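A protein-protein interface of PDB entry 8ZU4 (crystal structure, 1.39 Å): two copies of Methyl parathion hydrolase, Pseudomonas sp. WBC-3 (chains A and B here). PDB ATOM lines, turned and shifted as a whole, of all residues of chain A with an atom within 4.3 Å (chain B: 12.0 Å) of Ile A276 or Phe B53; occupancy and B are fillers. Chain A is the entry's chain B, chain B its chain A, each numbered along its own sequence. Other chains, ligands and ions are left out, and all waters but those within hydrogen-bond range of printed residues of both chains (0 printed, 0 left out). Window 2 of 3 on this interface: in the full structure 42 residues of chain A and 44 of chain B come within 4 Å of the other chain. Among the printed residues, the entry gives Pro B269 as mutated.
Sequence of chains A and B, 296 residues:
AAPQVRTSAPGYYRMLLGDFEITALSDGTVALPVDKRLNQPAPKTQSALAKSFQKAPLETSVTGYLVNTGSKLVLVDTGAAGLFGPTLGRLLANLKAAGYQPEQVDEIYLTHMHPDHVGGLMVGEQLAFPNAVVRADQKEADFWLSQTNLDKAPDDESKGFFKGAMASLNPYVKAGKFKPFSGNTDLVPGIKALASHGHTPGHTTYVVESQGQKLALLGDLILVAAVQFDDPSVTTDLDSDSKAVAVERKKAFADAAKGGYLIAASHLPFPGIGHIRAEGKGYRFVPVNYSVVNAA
The backbone carbonyl oxygen (O) of Lys B51 sits at hydrogen-bond distance from the guanidinium group (NE) of Arg A277 (3.2 Å).
The backbone carbonyl oxygen (O) of His A275 is in hydrogen-bond range of the backbone NH (N) of Val A286, at 2.8 Å. O of Arg A277 is in hydrogen-bond range of N of Arg A284 (2.8 Å).
Among the printed residues, merely in contact across the chains: His A275 with Phe B53 (3.5 Å), Ile A276 with Phe B53 (3.7 Å), Arg A284 with Arg B284 (3.7 Å) and Arg A277 with Ser B52 (3.8 Å).
Of chain B, only Phe B53 comes within 4 Å of Ile A276. Phe B53 touches two residues of chain A. No residue of chain B comes within 4 Å of Phe A229. No residue of chain B comes within 4 Å of Ala A257. No residue of chain B comes within 4 Å of Gly A260. No residue of chain B comes within 4 Å of Ile A263. Arg A277 touches just these residues of chain B: Lys B51 and Ser B52. No residue of chain B comes within 4 Å of Tyr A283. Printed residues of chain A within 4 Å of Lys B51: Arg A277 (3.2 Å). Printed residues of chain A within 4 Å of Ser B52: Arg A277 (3.8 Å). Printed residues of chain B within 4 Å of Arg A284: Arg B284. The nearest residue of chain A that does not touch Phe B53 is Val A286 (4.1 Å). The nearest printed residue of chain A that does not touch Arg B284 is Arg A277 (4.4 Å).
Of the 25 printed residues of chain B, 4 touch a printed residue of chain A. Hydrophobic or aromatic side chains of chain B within 4 Å of the printed part of chain A: Phe B53. Of the 12 printed residues of chain A, 4 touch a printed residue of chain B. Printed residues of chain A that touch a printed residue of chain B: His A275, Ile A276, Arg A277 and Arg A284. Hydrophobic or aromatic side chains of chain A within 4 Å of the printed part of chain B: His A275. Among the printed residues, 5 pairs touch across the chains.
Arg A284 touches its own counterpart, Arg B284.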
ATOM      1  N   PHE A 229      13.188   3.721  -9.956  1.00  0.00           N
ATOM      2  CA  PHE A 229      14.047   2.621  -9.532  1.00  0.00           C
ATOM      3  C   PHE A 229      13.451   1.283  -9.938  1.00  0.00           C
ATOM      4  O   PHE A 229      14.158   0.400 -10.440  1.00  0.00           O
ATOM      5  CB  PHE A 229      14.284   2.667  -8.021  1.00  0.00           C
ATOM      6  CG  PHE A 229      15.278   3.712  -7.602  1.00  0.00           C
ATOM      7  CD1 PHE A 229      16.595   3.657  -8.048  1.00  0.00           C
ATOM      8  CD2 PHE A 229      14.904   4.748  -6.756  1.00  0.00           C
ATOM      9  CE1 PHE A 229      17.514   4.625  -7.665  1.00  0.00           C
ATOM     10  CE2 PHE A 229      15.822   5.711  -6.365  1.00  0.00           C
ATOM     11  CZ  PHE A 229      17.131   5.647  -6.819  1.00  0.00           C
ATOM     12  N   ALA A 256      26.476   1.122 -10.277  1.00  0.00           N
ATOM     13  CA  ALA A 256      26.420   1.296  -8.830  1.00  0.00           C
ATOM     14  C   ALA A 256      26.068  -0.013  -8.126  1.00  0.00           C
ATOM     15  O   ALA A 256      26.613  -0.321  -7.057  1.00  0.00           O
ATOM     16  CB  ALA A 256      25.414   2.394  -8.483  1.00  0.00           C
ATOM     17  N   ALA A 257      25.152  -0.797  -8.705  1.00  0.00           N
ATOM     18  CA  ALA A 257      24.795  -2.077  -8.107  1.00  0.00           C
ATOM     19  C   ALA A 257      25.982  -3.035  -8.122  1.00  0.00           C
ATOM     20  O   ALA A 257      26.292  -3.670  -7.107  1.00  0.00           O
ATOM     21  CB  ALA A 257      23.594  -2.679  -8.837  1.00  0.00           C
ATOM     22  N   GLY A 260      28.751  -1.585  -5.722  1.00  0.00           N
ATOM     23  CA  GLY A 260      28.390  -1.425  -4.328  1.00  0.00           C
ATOM     24  C   GLY A 260      28.715  -0.076  -3.724  1.00  0.00           C
ATOM     25  O   GLY A 260      28.882   0.015  -2.504  1.00  0.00           O
ATOM     26  N   ILE A 263      25.429   6.445  -4.492  1.00  0.00           N
ATOM     27  CA  ILE A 263      24.987   7.417  -5.474  1.00  0.00           C
ATOM     28  C   ILE A 263      24.215   8.496  -4.738  1.00  0.00           C
ATOM     29  O   ILE A 263      23.741   8.307  -3.616  1.00  0.00           O
ATOM     30  CB  ILE A 263      24.091   6.820  -6.569  1.00  0.00           C
ATOM     31  CG1 ILE A 263      22.780   6.335  -5.940  1.00  0.00           C
ATOM     32  CG2 ILE A 263      24.823   5.692  -7.279  1.00  0.00           C
ATOM     33  CD1 ILE A 263      21.714   6.084  -6.956  1.00  0.00           C
ATOM     34  N   HIS A 275      22.918   3.488  -1.410  1.00  0.00           N
ATOM     35  CA  HIS A 275      23.385   2.423  -2.287  1.00  0.00           C
ATOM     36  C   HIS A 275      22.248   1.931  -3.181  1.00  0.00           C
ATOM     37  O   HIS A 275      21.084   2.297  -3.016  1.00  0.00           O
ATOM     38  CB  HIS A 275      23.926   1.241  -1.481  1.00  0.00           C
ATOM     39  CG  HIS A 275      25.151   1.549  -0.676  1.00  0.00           C
ATOM     40  ND1 HIS A 275      25.094   2.028   0.615  1.00  0.00           N
ATOM     41  CD2 HIS A 275      26.466   1.431  -0.976  1.00  0.00           C
ATOM     42  CE1 HIS A 275      26.322   2.194   1.075  1.00  0.00           C
ATOM     43  NE2 HIS A 275      27.174   1.839   0.128  1.00  0.00           N
ATOM     44  N   ILE A 276      22.597   1.082  -4.143  1.00  0.00           N
ATOM     45  CA  ILE A 276      21.634   0.497  -5.067  1.00  0.00           C
ATOM     46  C   ILE A 276      21.867  -0.997  -5.153  1.00  0.00           C
ATOM     47  O   ILE A 276      23.012  -1.452  -5.266  1.00  0.00           O
ATOM     48  CB  ILE A 276      21.715   1.115  -6.480  1.00  0.00           C
ATOM     49  CG1 ILE A 276      21.639   2.627  -6.400  1.00  0.00           C
ATOM     50  CG2 ILE A 276      20.639   0.527  -7.394  1.00  0.00           C
ATOM     51  CD1 ILE A 276      20.222   3.098  -6.500  1.00  0.00           C
ATOM     52  N   ARG A 277      20.786  -1.766  -5.109  1.00  0.00           N
ATOM     53  CA  ARG A 277      20.896  -3.178  -5.428  1.00  0.00           C
ATOM     54  C   ARG A 277      19.950  -3.556  -6.557  1.00  0.00           C
ATOM     55  O   ARG A 277      18.823  -3.062  -6.631  1.00  0.00           O
ATOM     56  CB  ARG A 277      20.799  -4.122  -4.206  1.00  0.00           C
ATOM     57  CG  ARG A 277      19.740  -3.828  -3.162  1.00  0.00           C
ATOM     58  CD  ARG A 277      19.396  -5.126  -2.415  1.00  0.00           C
ATOM     59  NE  ARG A 277      19.307  -4.933  -0.972  1.00  0.00           N
ATOM     60  CZ  ARG A 277      18.247  -4.460  -0.330  1.00  0.00           C
ATOM     61  NH1 ARG A 277      17.110  -4.215  -0.959  1.00  0.00           N
ATOM     62  NH2 ARG A 277      18.324  -4.249   0.982  1.00  0.00           N
ATOM     63  N   TYR A 283      15.678  -1.869  -9.743  1.00  0.00           N
ATOM     64  CA  TYR A 283      16.639  -1.575  -8.695  1.00  0.00           C
ATOM     65  C   TYR A 283      15.908  -1.141  -7.434  1.00  0.00           C
ATOM     66  O   TYR A 283      14.758  -0.696  -7.473  1.00  0.00           O
ATOM     67  CB  TYR A 283      17.646  -0.509  -9.161  1.00  0.00           C
ATOM     68  CG  TYR A 283      18.440  -0.976 -10.357  1.00  0.00           C
ATOM     69  CD1 TYR A 283      17.963  -0.800 -11.650  1.00  0.00           C
ATOM     70  CD2 TYR A 283      19.647  -1.642 -10.186  1.00  0.00           C
ATOM     71  CE1 TYR A 283      18.682  -1.259 -12.740  1.00  0.00           C
ATOM     72  CE2 TYR A 283      20.367  -2.100 -11.261  1.00  0.00           C
ATOM     73  CZ  TYR A 283      19.887  -1.907 -12.532  1.00  0.00           C
ATOM     74  OH  TYR A 283      20.622  -2.368 -13.591  1.00  0.00           O
ATOM     75  N   ARG A 284      16.595  -1.316  -6.309  1.00  0.00           N
ATOM     76  CA  ARG A 284      16.147  -0.891  -4.993  1.00  0.00           C
ATOM     77  C   ARG A 284      17.175   0.106  -4.470  1.00  0.00           C
ATOM     78  O   ARG A 284      18.375  -0.200  -4.421  1.00  0.00           O
ATOM     79  CB  ARG A 284      16.125  -2.102  -4.060  1.00  0.00           C
ATOM     80  CG  ARG A 284      16.018  -1.769  -2.581  1.00  0.00           C
ATOM     81  CD  ARG A 284      14.591  -1.525  -2.145  1.00  0.00           C
ATOM     82  NE  ARG A 284      13.679  -2.440  -2.819  1.00  0.00           N
ATOM     83  CZ  ARG A 284      12.373  -2.251  -2.944  1.00  0.00           C
ATOM     84  NH1 ARG A 284      11.770  -1.209  -2.395  1.00  0.00           N
ATOM     85  NH2 ARG A 284      11.653  -3.134  -3.631  1.00  0.00           N
ATOM     86  N   PHE A 285      16.709   1.294  -4.094  1.00  0.00           N
ATOM     87  CA  PHE A 285      17.556   2.314  -3.487  1.00  0.00           C
ATOM     88  C   PHE A 285      17.574   2.079  -1.982  1.00  0.00           C
ATOM     89  O   PHE A 285      16.525   1.848  -1.372  1.00  0.00           O
ATOM     90  CB  PHE A 285      16.981   3.698  -3.798  1.00  0.00           C
ATOM     91  CG  PHE A 285      17.756   4.839  -3.209  1.00  0.00           C
ATOM     92  CD1 PHE A 285      19.067   5.081  -3.590  1.00  0.00           C
ATOM     93  CD2 PHE A 285      17.156   5.704  -2.302  1.00  0.00           C
ATOM     94  CE1 PHE A 285      19.776   6.150  -3.056  1.00  0.00           C
ATOM     95  CE2 PHE A 285      17.856   6.772  -1.765  1.00  0.00           C
ATOM     96  CZ  PHE A 285      19.174   6.990  -2.136  1.00  0.00           C
ATOM     97  N   VAL A 286      18.759   2.118  -1.392  1.00  0.00           N
ATOM     98  CA  VAL A 286      18.951   1.895   0.031  1.00  0.00           C
ATOM     99  C   VAL A 286      19.567   3.157   0.622  1.00  0.00           C
ATOM    100  O   VAL A 286      20.776   3.373   0.530  1.00  0.00           O
ATOM    101  CB  VAL A 286      19.836   0.662   0.291  1.00  0.00           C
ATOM    102  CG1 VAL A 286      19.960   0.391   1.784  1.00  0.00           C
ATOM    103  CG2 VAL A 286      19.256  -0.562  -0.421  1.00  0.00           C
ATOM    104  N   VAL B  34      25.489  -5.944  17.327  1.00  0.00           N
ATOM    105  CA  VAL B  34      24.187  -6.584  17.169  1.00  0.00           C
ATOM    106  C   VAL B  34      24.323  -8.056  16.802  1.00  0.00           C
ATOM    107  O   VAL B  34      23.416  -8.848  17.088  1.00  0.00           O
ATOM    108  CB  VAL B  34      23.291  -5.801  16.189  1.00  0.00           C
ATOM    109  CG1 VAL B  34      23.090  -4.385  16.694  1.00  0.00           C
ATOM    110  CG2 VAL B  34      23.888  -5.802  14.795  1.00  0.00           C
ATOM    111  N   LYS B  44      24.792 -15.254  10.226  1.00  0.00           N
ATOM    112  CA  LYS B  44      23.482 -14.952   9.652  1.00  0.00           C
ATOM    113  C   LYS B  44      23.147 -13.472   9.804  1.00  0.00           C
ATOM    114  O   LYS B  44      22.706 -12.814   8.849  1.00  0.00           O
ATOM    115  CB  LYS B  44      22.430 -15.819  10.344  1.00  0.00           C
ATOM    116  CG  LYS B  44      21.058 -15.805   9.706  1.00  0.00           C
ATOM    117  CD  LYS B  44      20.101 -16.662  10.532  1.00  0.00           C
ATOM    118  CE  LYS B  44      19.121 -17.424   9.667  1.00  0.00           C
ATOM    119  NZ  LYS B  44      17.912 -16.599   9.380  1.00  0.00           N
ATOM    120  N   THR B  45      23.365 -12.927  10.999  1.00  0.00           N
ATOM    121  CA  THR B  45      23.192 -11.496  11.189  1.00  0.00           C
ATOM    122  C   THR B  45      24.102 -10.714  10.256  1.00  0.00           C
ATOM    123  O   THR B  45      23.663  -9.754   9.615  1.00  0.00           O
ATOM    124  CB  THR B  45      23.466 -11.130  12.649  1.00  0.00           C
ATOM    125  OG1 THR B  45      22.439 -11.696  13.462  1.00  0.00           O
ATOM    126  CG2 THR B  45      23.477  -9.611  12.842  1.00  0.00           C
ATOM    127  N   GLN B  46      25.369 -11.120  10.152  1.00  0.00           N
ATOM    128  CA  GLN B  46      26.311 -10.364   9.332  1.00  0.00           C
ATOM    129  C   GLN B  46      25.892 -10.359   7.864  1.00  0.00           C
ATOM    130  O   GLN B  46      26.017  -9.337   7.182  1.00  0.00           O
ATOM    131  CB  GLN B  46      27.726 -10.913   9.503  1.00  0.00           C
ATOM    132  CG  GLN B  46      28.387 -10.462  10.811  1.00  0.00           C
ATOM    133  CD  GLN B  46      28.858  -9.010  10.798  1.00  0.00           C
ATOM    134  OE1 GLN B  46      28.076  -8.082  10.559  1.00  0.00           O
ATOM    135  NE2 GLN B  46      30.142  -8.808  11.084  1.00  0.00           N
ATOM    136  N   SER B  47      25.396 -11.492   7.358  1.00  0.00           N
ATOM    137  CA  SER B  47      24.954 -11.550   5.964  1.00  0.00           C
ATOM    138  C   SER B  47      23.681 -10.729   5.745  1.00  0.00           C
ATOM    139  O   SER B  47      23.532 -10.050   4.710  1.00  0.00           O
ATOM    140  CB  SER B  47      24.782 -13.007   5.526  1.00  0.00           C
ATOM    141  OG  SER B  47      23.592 -13.566   6.056  1.00  0.00           O
ATOM    142  N   ALA B  48      22.761 -10.755   6.719  1.00  0.00           N
ATOM    143  CA  ALA B  48      21.589  -9.887   6.635  1.00  0.00           C
ATOM    144  C   ALA B  48      21.997  -8.419   6.604  1.00  0.00           C
ATOM    145  O   ALA B  48      21.447  -7.627   5.829  1.00  0.00           O
ATOM    146  CB  ALA B  48      20.645 -10.153   7.804  1.00  0.00           C
ATOM    147  N   LEU B  49      22.959  -8.039   7.441  1.00  0.00           N
ATOM    148  CA  LEU B  49      23.450  -6.665   7.436  1.00  0.00           C
ATOM    149  C   LEU B  49      24.100  -6.326   6.102  1.00  0.00           C
ATOM    150  O   LEU B  49      23.874  -5.243   5.549  1.00  0.00           O
ATOM    151  CB  LEU B  49      24.443  -6.464   8.580  1.00  0.00           C
ATOM    152  CG  LEU B  49      23.847  -6.469   9.997  1.00  0.00           C
ATOM    153  CD1 LEU B  49      24.882  -6.019  11.017  1.00  0.00           C
ATOM    154  CD2 LEU B  49      22.592  -5.626  10.093  1.00  0.00           C
ATOM    155  N   ALA B  50      24.897  -7.253   5.556  1.00  0.00           N
ATOM    156  CA  ALA B  50      25.567  -7.004   4.284  1.00  0.00           C
ATOM    157  C   ALA B  50      24.563  -6.726   3.175  1.00  0.00           C
ATOM    158  O   ALA B  50      24.828  -5.907   2.281  1.00  0.00           O
ATOM    159  CB  ALA B  50      26.471  -8.179   3.904  1.00  0.00           C
ATOM    160  N   LYS B  51      23.407  -7.407   3.201  1.00  0.00           N
ATOM    161  CA  LYS B  51      22.381  -7.115   2.196  1.00  0.00           C
ATOM    162  C   LYS B  51      21.988  -5.644   2.206  1.00  0.00           C
ATOM    163  O   LYS B  51      21.655  -5.084   1.155  1.00  0.00           O
ATOM    164  CB  LYS B  51      21.129  -7.968   2.404  1.00  0.00           C
ATOM    165  CG  LYS B  51      21.247  -9.432   2.028  1.00  0.00           C
ATOM    166  CD  LYS B  51      19.920 -10.127   2.320  1.00  0.00           C
ATOM    167  CE  LYS B  51      20.027 -11.632   2.236  1.00  0.00           C
ATOM    168  NZ  LYS B  51      18.697 -12.262   2.481  1.00  0.00           N
ATOM    169  N   SER B  52      22.023  -5.002   3.373  1.00  0.00           N
ATOM    170  CA  SER B  52      21.686  -3.594   3.510  1.00  0.00           C
ATOM    171  C   SER B  52      22.921  -2.702   3.571  1.00  0.00           C
ATOM    172  O   SER B  52      22.827  -1.561   4.040  1.00  0.00           O
ATOM    173  CB  SER B  52      20.798  -3.378   4.736  1.00  0.00           C
ATOM    174  OG  SER B  52      19.522  -3.971   4.542  1.00  0.00           O
ATOM    175  N   PHE B  53      24.071  -3.199   3.111  1.00  0.00           N
ATOM    176  CA  PHE B  53      25.315  -2.420   3.084  1.00  0.00           C
ATOM    177  C   PHE B  53      25.746  -1.981   4.488  1.00  0.00           C
ATOM    178  O   PHE B  53      26.300  -0.896   4.678  1.00  0.00           O
ATOM    179  CB  PHE B  53      25.217  -1.235   2.115  1.00  0.00           C
ATOM    180  CG  PHE B  53      24.776  -1.630   0.732  1.00  0.00           C
ATOM    181  CD1 PHE B  53      23.424  -1.679   0.401  1.00  0.00           C
ATOM    182  CD2 PHE B  53      25.712  -1.964  -0.230  1.00  0.00           C
ATOM    183  CE1 PHE B  53      23.020  -2.058  -0.881  1.00  0.00           C
ATOM    184  CE2 PHE B  53      25.315  -2.338  -1.511  1.00  0.00           C
ATOM    185  CZ  PHE B  53      23.967  -2.385  -1.830  1.00  0.00           C
ATOM    186  N   GLN B  54      25.491  -2.851   5.449  1.00  0.00           N
ATOM    187  CA  GLN B  54      25.855  -2.592   6.820  1.00  0.00           C
ATOM    188  C   GLN B  54      26.727  -3.709   7.365  1.00  0.00           C
ATOM    189  O   GLN B  54      26.813  -4.753   6.773  1.00  0.00           O
ATOM    190  CB  GLN B  54      24.585  -2.473   7.696  1.00  0.00           C
ATOM    191  CG  GLN B  54      23.705  -1.270   7.405  1.00  0.00           C
ATOM    192  CD  GLN B  54      22.331  -1.376   8.038  1.00  0.00           C
ATOM    193  OE1 GLN B  54      22.093  -2.224   8.883  1.00  0.00           O
ATOM    194  NE2 GLN B  54      21.423  -0.513   7.624  1.00  0.00           N
ATOM    195  N   LYS B  55      27.453  -3.422   8.423  1.00  0.00           N
ATOM    196  CA  LYS B  55      28.263  -4.425   9.081  1.00  0.00           C
ATOM    197  C   LYS B  55      28.250  -4.152  10.588  1.00  0.00           C
ATOM    198  O   LYS B  55      28.125  -3.018  10.991  1.00  0.00           O
ATOM    199  CB  LYS B  55      29.667  -4.367   8.529  1.00  0.00           C
ATOM    200  CG  LYS B  55      30.539  -5.522   8.983  1.00  0.00           C
ATOM    201  CD  LYS B  55      31.759  -5.683   8.089  1.00  0.00           C
ATOM    202  CE  LYS B  55      31.360  -6.126   6.690  1.00  0.00           C
ATOM    203  NZ  LYS B  55      32.517  -6.181   5.754  1.00  0.00           N
ATOM    204  N   ALA B  56      28.284  -5.183  11.409  1.00  0.00           N
ATOM    205  CA  ALA B  56      28.398  -4.996  12.846  1.00  0.00           C
ATOM    206  C   ALA B  56      29.848  -4.738  13.156  1.00  0.00           C
ATOM    207  O   ALA B  56      30.693  -5.282  12.478  1.00  0.00           O
ATOM    208  CB  ALA B  56      27.851  -6.185  13.585  1.00  0.00           C
ATOM    209  N   PRO B  57      30.162  -3.938  14.169  1.00  0.00           N
ATOM    210  CA  PRO B  57      29.265  -3.155  15.019  1.00  0.00           C
ATOM    211  C   PRO B  57      28.511  -2.123  14.211  1.00  0.00           C
ATOM    212  O   PRO B  57      29.074  -1.466  13.362  1.00  0.00           O
ATOM    213  CB  PRO B  57      30.202  -2.499  16.029  1.00  0.00           C
ATOM    214  CG  PRO B  57      31.541  -2.532  15.389  1.00  0.00           C
ATOM    215  CD  PRO B  57      31.564  -3.784  14.576  1.00  0.00           C
ATOM    216  N   LEU B  58      27.247  -1.957  14.535  1.00  0.00           N
ATOM    217  CA  LEU B  58      26.400  -1.114  13.737  1.00  0.00           C
ATOM    218  C   LEU B  58      26.060   0.176  14.449  1.00  0.00           C
ATOM    219  O   LEU B  58      25.573   0.159  15.550  1.00  0.00           O
ATOM    220  CB  LEU B  58      25.135  -1.902  13.486  1.00  0.00           C
ATOM    221  CG  LEU B  58      24.044  -1.328  12.605  1.00  0.00           C
ATOM    222  CD1 LEU B  58      24.630  -1.062  11.235  1.00  0.00           C
ATOM    223  CD2 LEU B  58      22.919  -2.341  12.518  1.00  0.00           C
ATOM    224  N   GLU B  59      26.300   1.282  13.770  1.00  0.00           N
ATOM    225  CA  GLU B  59      25.991   2.535  14.375  1.00  0.00           C
ATOM    226  C   GLU B  59      24.482   2.577  14.460  1.00  0.00           C
ATOM    227  O   GLU B  59      23.816   2.550  13.455  1.00  0.00           O
ATOM    228  CB  GLU B  59      26.530   3.670  13.519  1.00  0.00           C
ATOM    229  CG  GLU B  59      26.235   5.051  14.058  1.00  0.00           C
ATOM    230  CD  GLU B  59      26.958   6.162  13.315  1.00  0.00           C
ATOM    231  OE1 GLU B  59      27.576   5.886  12.276  1.00  0.00           O
ATOM    232  OE2 GLU B  59      26.895   7.314  13.772  1.00  0.00           O
ATOM    233  N   THR B  60      23.980   2.824  15.650  1.00  0.00           N
ATOM    234  CA  THR B  60      22.554   2.737  15.893  1.00  0.00           C
ATOM    235  C   THR B  60      22.045   4.031  16.517  1.00  0.00           C
ATOM    236  O   THR B  60      22.628   4.530  17.444  1.00  0.00           O
ATOM    237  CB  THR B  60      22.282   1.534  16.819  1.00  0.00           C
ATOM    238  OG1 THR B  60      22.720   0.320  16.207  1.00  0.00           O
ATOM    239  CG2 THR B  60      20.796   1.421  17.145  1.00  0.00           C
ATOM    240  N   VAL B 224      16.902  -3.807  15.276  1.00  0.00           N
ATOM    241  CA  VAL B 224      17.841  -3.888  14.160  1.00  0.00           C
ATOM    242  C   VAL B 224      16.999  -3.959  12.896  1.00  0.00           C
ATOM    243  O   VAL B 224      16.517  -5.034  12.525  1.00  0.00           O
ATOM    244  CB  VAL B 224      18.775  -5.099  14.267  1.00  0.00           C
ATOM    245  CG1 VAL B 224      19.854  -5.017  13.205  1.00  0.00           C
ATOM    246  CG2 VAL B 224      19.395  -5.180  15.658  1.00  0.00           C
ATOM    247  N   ALA B 225      16.842  -2.822  12.213  1.00  0.00           N
ATOM    248  CA  ALA B 225      15.956  -2.764  11.048  1.00  0.00           C
ATOM    249  C   ALA B 225      16.359  -3.768   9.974  1.00  0.00           C
ATOM    250  O   ALA B 225      15.496  -4.434   9.384  1.00  0.00           O
ATOM    251  CB  ALA B 225      15.923  -1.347  10.475  1.00  0.00           C
ATOM    252  N   ALA B 226      17.663  -3.906   9.711  1.00  0.00           N
ATOM    253  CA  ALA B 226      18.126  -4.764   8.623  1.00  0.00           C
ATOM    254  C   ALA B 226      17.920  -6.251   8.895  1.00  0.00           C
ATOM    255  O   ALA B 226      18.119  -7.062   7.981  1.00  0.00           O
ATOM    256  CB  ALA B 226      19.595  -4.483   8.301  1.00  0.00           C
ATOM    257  N   VAL B 227      17.539  -6.632  10.113  1.00  0.00           N
ATOM    258  CA  VAL B 227      17.258  -8.019  10.459  1.00  0.00           C
ATOM    259  C   VAL B 227      15.772  -8.239  10.728  1.00  0.00           C
ATOM    260  O   VAL B 227      15.163  -9.162  10.183  1.00  0.00           O
ATOM    261  CB  VAL B 227      18.121  -8.488  11.652  1.00  0.00           C
ATOM    262  CG1 VAL B 227      17.617  -9.832  12.191  1.00  0.00           C
ATOM    263  CG2 VAL B 227      19.588  -8.573  11.249  1.00  0.00           C
ATOM    264  N   ASP B 230      12.584  -8.008   7.962  1.00  0.00           N
ATOM    265  CA  ASP B 230      12.512  -9.184   7.102  1.00  0.00           C
ATOM    266  C   ASP B 230      12.118 -10.418   7.901  1.00  0.00           C
ATOM    267  O   ASP B 230      11.405 -11.291   7.392  1.00  0.00           O
ATOM    268  CB  ASP B 230      13.875  -9.420   6.452  1.00  0.00           C
ATOM    269  CG  ASP B 230      14.151  -8.473   5.299  1.00  0.00           C
ATOM    270  OD1 ASP B 230      13.188  -7.889   4.758  1.00  0.00           O
ATOM    271  OD2 ASP B 230      15.338  -8.314   4.938  1.00  0.00           O
ATOM    272  N   PRO B 269      16.939   4.072  12.091  1.00  0.00           N
ATOM    273  CA  PRO B 269      17.844   5.173  11.747  1.00  0.00           C
ATOM    274  C   PRO B 269      17.106   6.501  11.821  1.00  0.00           C
ATOM    275  O   PRO B 269      16.027   6.657  11.244  1.00  0.00           O
ATOM    276  CB  PRO B 269      18.260   4.845  10.310  1.00  0.00           C
ATOM    277  CG  PRO B 269      18.122   3.340  10.219  1.00  0.00           C
ATOM    278  CD  PRO B 269      16.908   3.022  11.054  1.00  0.00           C
ATOM    279  N   ARG B 284       8.485  -4.552   4.951  1.00  0.00           N
ATOM    280  CA  ARG B 284       9.394  -3.546   4.430  1.00  0.00           C
ATOM    281  C   ARG B 284       9.045  -2.222   5.086  1.00  0.00           C
ATOM    282  O   ARG B 284       7.879  -1.804   5.072  1.00  0.00           O
ATOM    283  CB  ARG B 284       9.274  -3.409   2.910  1.00  0.00           C
ATOM    284  CG  ARG B 284      10.067  -2.236   2.349  1.00  0.00           C
ATOM    285  CD  ARG B 284      10.319  -2.363   0.858  1.00  0.00           C
ATOM    286  NE  ARG B 284      11.104  -3.539   0.496  1.00  0.00           N
ATOM    287  CZ  ARG B 284      12.391  -3.703   0.771  1.00  0.00           C
ATOM    288  NH1 ARG B 284      13.081  -2.786   1.432  1.00  0.00           N
ATOM    289  NH2 ARG B 284      13.004  -4.812   0.365  1.00  0.00           N
